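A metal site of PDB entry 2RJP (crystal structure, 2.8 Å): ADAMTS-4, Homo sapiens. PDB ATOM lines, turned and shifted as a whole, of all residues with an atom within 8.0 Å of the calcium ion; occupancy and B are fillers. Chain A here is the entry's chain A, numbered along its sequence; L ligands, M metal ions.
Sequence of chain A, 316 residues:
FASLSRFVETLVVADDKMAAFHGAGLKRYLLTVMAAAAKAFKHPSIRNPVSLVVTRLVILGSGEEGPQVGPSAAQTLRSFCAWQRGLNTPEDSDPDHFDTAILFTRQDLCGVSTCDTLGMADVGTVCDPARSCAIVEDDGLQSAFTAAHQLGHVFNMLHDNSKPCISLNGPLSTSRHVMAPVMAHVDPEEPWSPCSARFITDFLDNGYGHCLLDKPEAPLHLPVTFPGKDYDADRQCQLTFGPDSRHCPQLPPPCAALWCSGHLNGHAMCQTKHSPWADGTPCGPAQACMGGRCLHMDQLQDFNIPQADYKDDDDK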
ATOM      1  N   PRO A  71      26.668  31.901   0.276  1.00  0.00           N
ATOM      2  CA  PRO A  71      26.435  32.153  -1.150  1.00  0.00           C
ATOM      3  C   PRO A  71      27.692  31.973  -2.007  1.00  0.00           C
ATOM      4  O   PRO A  71      27.581  31.557  -3.154  1.00  0.00           O
ATOM      5  CB  PRO A  71      25.943  33.607  -1.189  1.00  0.00           C
ATOM      6  CG  PRO A  71      25.636  33.967   0.244  1.00  0.00           C
ATOM      7  CD  PRO A  71      26.581  33.150   1.064  1.00  0.00           C
ATOM      8  N   ALA A  73      30.434  30.200  -3.711  1.00  0.00           N
ATOM      9  CA  ALA A  73      30.730  28.824  -4.106  1.00  0.00           C
ATOM     10  C   ALA A  73      32.190  28.440  -3.842  1.00  0.00           C
ATOM     11  O   ALA A  73      32.482  27.341  -3.370  1.00  0.00           O
ATOM     12  CB  ALA A  73      30.362  28.576  -5.569  1.00  0.00           C
ATOM     13  N   GLN A 107      21.008  25.742  -0.780  1.00  0.00           N
ATOM     14  CA  GLN A 107      21.584  27.094  -0.798  1.00  0.00           C
ATOM     15  C   GLN A 107      21.845  27.547  -2.223  1.00  0.00           C
ATOM     16  O   GLN A 107      22.389  26.780  -3.031  1.00  0.00           O
ATOM     17  CB  GLN A 107      22.889  27.092   0.002  1.00  0.00           C
ATOM     18  CG  GLN A 107      23.838  28.253  -0.291  1.00  0.00           C
ATOM     19  CD  GLN A 107      23.356  29.551   0.303  1.00  0.00           C
ATOM     20  OE1 GLN A 107      23.005  29.615   1.478  1.00  0.00           O
ATOM     21  NE2 GLN A 107      23.328  30.592  -0.513  1.00  0.00           N
ATOM     22  N   ASP A 108      21.452  28.775  -2.541  1.00  0.00           N
ATOM     23  CA  ASP A 108      21.754  29.326  -3.855  1.00  0.00           C
ATOM     24  C   ASP A 108      23.238  29.648  -3.943  1.00  0.00           C
ATOM     25  O   ASP A 108      23.684  30.712  -3.494  1.00  0.00           O
ATOM     26  CB  ASP A 108      20.895  30.552  -4.185  1.00  0.00           C
ATOM     27  CG  ASP A 108      21.079  31.029  -5.629  1.00  0.00           C
ATOM     28  OD1 ASP A 108      21.633  30.265  -6.448  1.00  0.00           O
ATOM     29  OD2 ASP A 108      20.659  32.160  -5.952  1.00  0.00           O
ATOM     30  N   LEU A 109      24.004  28.709  -4.504  1.00  0.00           N
ATOM     31  CA  LEU A 109      25.443  28.853  -4.694  1.00  0.00           C
ATOM     32  C   LEU A 109      25.726  29.877  -5.766  1.00  0.00           C
ATOM     33  O   LEU A 109      25.076  29.904  -6.814  1.00  0.00           O
ATOM     34  CB  LEU A 109      26.115  27.514  -5.047  1.00  0.00           C
ATOM     35  CG  LEU A 109      26.149  26.412  -3.978  1.00  0.00           C
ATOM     36  CD1 LEU A 109      26.896  25.204  -4.522  1.00  0.00           C
ATOM     37  CD2 LEU A 109      26.767  26.875  -2.647  1.00  0.00           C
ATOM     38  N   CYS A 110      26.706  30.731  -5.492  1.00  0.00           N
ATOM     39  CA  CYS A 110      26.916  31.912  -6.294  1.00  0.00           C
ATOM     40  C   CYS A 110      28.413  32.138  -6.572  1.00  0.00           C
ATOM     41  O   CYS A 110      29.231  32.105  -5.649  1.00  0.00           O
ATOM     42  CB  CYS A 110      26.305  33.105  -5.564  1.00  0.00           C
ATOM     43  SG  CYS A 110      25.847  34.448  -6.632  1.00  0.00           S
ATOM     44  N   GLY A 111      28.754  32.319  -7.850  1.00  0.00           N
ATOM     45  CA  GLY A 111      30.128  32.574  -8.289  1.00  0.00           C
ATOM     46  C   GLY A 111      30.586  34.012  -8.057  1.00  0.00           C
ATOM     47  O   GLY A 111      29.961  34.742  -7.281  1.00  0.00           O
ATOM     48  N   THR A 114      27.933  36.139 -11.106  1.00  0.00           N
ATOM     49  CA  THR A 114      26.497  35.860 -11.087  1.00  0.00           C
ATOM     50  C   THR A 114      26.153  34.688 -10.157  1.00  0.00           C
ATOM     51  O   THR A 114      27.055  34.001  -9.676  1.00  0.00           O
ATOM     52  CB  THR A 114      25.954  35.599 -12.521  1.00  0.00           C
ATOM     53  OG1 THR A 114      24.585  35.161 -12.456  1.00  0.00           O
ATOM     54  CG2 THR A 114      26.794  34.539 -13.255  1.00  0.00           C
ATOM     55  N   CYS A 115      24.863  34.495  -9.905  1.00  0.00           N
ATOM     56  CA  CYS A 115      24.371  33.382  -9.082  1.00  0.00           C
ATOM     57  C   CYS A 115      23.903  32.187  -9.911  1.00  0.00           C
ATOM     58  O   CYS A 115      23.423  31.195  -9.354  1.00  0.00           O
ATOM     59  CB  CYS A 115      23.259  33.855  -8.128  1.00  0.00           C
ATOM     60  SG  CYS A 115      23.827  34.535  -6.528  1.00  0.00           S
ATOM     61  N   ASP A 116      24.056  32.269 -11.236  1.00  0.00           N
ATOM     62  CA  ASP A 116      23.735  31.150 -12.146  1.00  0.00           C
ATOM     63  C   ASP A 116      24.642  29.933 -11.915  1.00  0.00           C
ATOM     64  O   ASP A 116      24.325  28.832 -12.371  1.00  0.00           O
ATOM     65  CB  ASP A 116      23.816  31.607 -13.607  1.00  0.00           C
ATOM     66  CG  ASP A 116      22.832  32.739 -13.938  1.00  0.00           C
ATOM     67  OD1 ASP A 116      21.715  32.752 -13.374  1.00  0.00           O
ATOM     68  OD2 ASP A 116      23.176  33.609 -14.760  1.00  0.00           O
ATOM     69  N   THR A 117      25.754  30.141 -11.223  1.00  0.00           N
ATOM     70  CA  THR A 117      26.618  29.040 -10.784  1.00  0.00           C
ATOM     71  C   THR A 117      25.798  27.926 -10.132  1.00  0.00           C
ATOM     72  O   THR A 117      24.962  28.198  -9.263  1.00  0.00           O
ATOM     73  CB  THR A 117      27.680  29.557  -9.794  1.00  0.00           C
ATOM     74  OG1 THR A 117      28.473  30.555 -10.428  1.00  0.00           O
ATOM     75  CG2 THR A 117      28.581  28.437  -9.293  1.00  0.00           C
ATOM     76  N   LEU A 118      26.023  26.690 -10.563  1.00  0.00           N
ATOM     77  CA  LEU A 118      25.287  25.542 -10.022  1.00  0.00           C
ATOM     78  C   LEU A 118      26.159  24.558  -9.228  1.00  0.00           C
ATOM     79  O   LEU A 118      25.635  23.660  -8.575  1.00  0.00           O
ATOM     80  CB  LEU A 118      24.496  24.828 -11.118  1.00  0.00           C
ATOM     81  CG  LEU A 118      23.210  25.544 -11.573  1.00  0.00           C
ATOM     82  CD1 LEU A 118      22.592  24.879 -12.774  1.00  0.00           C
ATOM     83  CD2 LEU A 118      22.188  25.626 -10.444  1.00  0.00           C
ATOM     84  N   GLY A 119      27.474  24.730  -9.286  1.00  0.00           N
ATOM     85  CA  GLY A 119      28.378  23.866  -8.534  1.00  0.00           C
ATOM     86  C   GLY A 119      29.839  24.192  -8.763  1.00  0.00           C
ATOM     87  O   GLY A 119      30.164  25.022  -9.594  1.00  0.00           O
ATOM     88  N   GLU A 137      24.555  22.629  -6.173  1.00  0.00           N
ATOM     89  CA  GLU A 137      23.326  23.307  -5.824  1.00  0.00           C
ATOM     90  C   GLU A 137      22.160  22.504  -6.372  1.00  0.00           C
ATOM     91  O   GLU A 137      22.027  22.314  -7.573  1.00  0.00           O
ATOM     92  CB  GLU A 137      23.294  24.727  -6.388  1.00  0.00           C
ATOM     93  CG  GLU A 137      21.984  25.450  -6.131  1.00  0.00           C
ATOM     94  CD  GLU A 137      21.905  26.797  -6.813  1.00  0.00           C
ATOM     95  OE1 GLU A 137      22.870  27.582  -6.705  1.00  0.00           O
ATOM     96  OE2 GLU A 137      20.880  27.069  -7.458  1.00  0.00           O
ATOM     97  N   ASP A 139      18.673  21.955  -7.492  1.00  0.00           N
ATOM     98  CA  ASP A 139      17.502  22.629  -8.023  1.00  0.00           C
ATOM     99  C   ASP A 139      16.594  21.624  -8.710  1.00  0.00           C
ATOM    100  O   ASP A 139      15.989  21.908  -9.746  1.00  0.00           O
ATOM    101  CB  ASP A 139      17.908  23.771  -8.967  1.00  0.00           C
ATOM    102  CG  ASP A 139      18.717  23.299 -10.183  1.00  0.00           C
ATOM    103  OD1 ASP A 139      19.323  22.204 -10.149  1.00  0.00           O
ATOM    104  OD2 ASP A 139      18.777  24.054 -11.183  1.00  0.00           O
ATOM    105  N   LYS A 273      12.997  26.224 -15.714  1.00  0.00           N
ATOM    106  CA  LYS A 273      14.450  26.360 -15.752  1.00  0.00           C
ATOM    107  C   LYS A 273      14.986  25.731 -17.037  1.00  0.00           C
ATOM    108  O   LYS A 273      16.183  25.469 -17.155  1.00  0.00           O
ATOM    109  CB  LYS A 273      15.127  25.721 -14.535  1.00  0.00           C
ATOM    110  CG  LYS A 273      15.021  26.555 -13.273  1.00  0.00           C
ATOM    111  CD  LYS A 273      16.085  26.231 -12.223  1.00  0.00           C
ATOM    112  CE  LYS A 273      15.939  27.197 -11.030  1.00  0.00           C
ATOM    113  NZ  LYS A 273      16.768  26.905  -9.817  1.00  0.00           N
HETATM  114  C1  LIG L   1      31.739  28.311 -11.418  1.00  0.00           C
HETATM  115  C2  LIG L   1      32.413  27.121 -12.132  1.00  0.00           C
HETATM  116  C3  LIG L   1      33.521  26.585 -11.214  1.00  0.00           C
HETATM  117  C4  LIG L   1      31.355  26.064 -12.505  1.00  0.00           C
HETATM  118  C5  LIG L   1      31.934  24.817 -13.268  1.00  0.00           C
HETATM  119  O1  LIG L   1      32.434  25.100 -14.393  1.00  0.00           O
HETATM  120  O2  LIG L   1      31.843  23.700 -12.717  1.00  0.00           O
HETATM  121  N1  LIG L   1      30.431  26.715 -13.510  1.00  0.00           N
HETATM  122  S1  LIG L   1      28.774  26.650 -13.223  1.00  0.00           S
HETATM  123  O3  LIG L   1      28.208  27.855 -13.825  1.00  0.00           O
HETATM  124  O4  LIG L   1      28.536  26.366 -11.822  1.00  0.00           O
HETATM  125  C6  LIG L   1      28.215  25.235 -14.138  1.00  0.00           C
HETATM  126  C7  LIG L   1      28.054  25.340 -15.520  1.00  0.00           C
HETATM  127  C8  LIG L   1      27.610  24.226 -16.238  1.00  0.00           C
HETATM  128  C9  LIG L   1      27.313  22.994 -15.600  1.00  0.00           C
HETATM  129  C10 LIG L   1      27.492  22.922 -14.202  1.00  0.00           C
HETATM  130  C11 LIG L   1      27.927  24.033 -13.473  1.00  0.00           C
HETATM  131  C12 LIG L   1      26.828  21.834 -16.386  1.00  0.00           C
HETATM  132  C13 LIG L   1      26.035  20.832 -15.781  1.00  0.00           C
HETATM  133  C14 LIG L   1      25.555  19.729 -16.517  1.00  0.00           C
HETATM  134  C15 LIG L   1      25.841  19.610 -17.886  1.00  0.00           C
HETATM  135  C16 LIG L   1      26.620  20.614 -18.501  1.00  0.00           C
HETATM  136  C17 LIG L   1      27.096  21.704 -17.763  1.00  0.00           C
HETATM  137  C18 LIG L   1      25.359  18.435 -18.711  1.00  0.00           C
HETATM  138  O5  LIG L   1      24.290  17.735 -18.066  1.00  0.00           O
HETATM  139  C19 LIG L   1      24.152  16.369 -18.065  1.00  0.00           C
HETATM  140  C20 LIG L   1      24.995  15.396 -17.501  1.00  0.00           C
HETATM  141  C21 LIG L   1      24.660  14.026 -17.581  1.00  0.00           C
HETATM  142  C22 LIG L   1      23.480  13.586 -18.210  1.00  0.00           C
HETATM  143  C23 LIG L   1      22.637  14.569 -18.752  1.00  0.00           C
HETATM  144  C24 LIG L   1      22.968  15.932 -18.678  1.00  0.00           C
HETATM  145  C25 LIG L   1      23.077  12.126 -18.288  1.00  0.00           C
HETATM  146  O6  LIG L   1      22.961  11.558 -17.203  1.00  0.00           O
HETATM  147  C26 LIG L   1      22.455  11.444 -19.518  1.00  0.00           C
HETATM  148  C27 LIG L   1      23.194  11.745 -20.815  1.00  0.00           C
HETATM  149  C28 LIG L   1      20.947  11.684 -19.630  1.00  0.00           C
HETATM  150 CA    CA M   1      23.273  29.412  -8.096  1.00  0.00          CA
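The backbone NH of Gly 119 sits at hydrogen-bond distance from an oxygen (O4) of the ligand.
O4 of the ligand lies within hydrogen-bond range of N of Leu 118.
N of Gly 111 lies within hydrogen-bond range of OG1 of Thr 117.
The backbone NH (N) of Glu 137 lies within hydrogen-bond range of the backbone carbonyl oxygen (O) of Leu 118 (2.8 Å).
SG of Cys 115 is disulfide-bonded to SG of Cys 110, at 2.0 Å.
Of the 16 residues printed, 5 come within 4 Å of the calcium ion.
The calcium ion is bound by O of Cys 115 (2.2 Å), O of Leu 109 (2.3 Å), OE1 of Glu 137 (2.3 Å), O of Thr 117 (2.4 Å) and OD1 of Asp 108 (2.5 Å).
The calcium ion has five donor atoms within binding distance.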
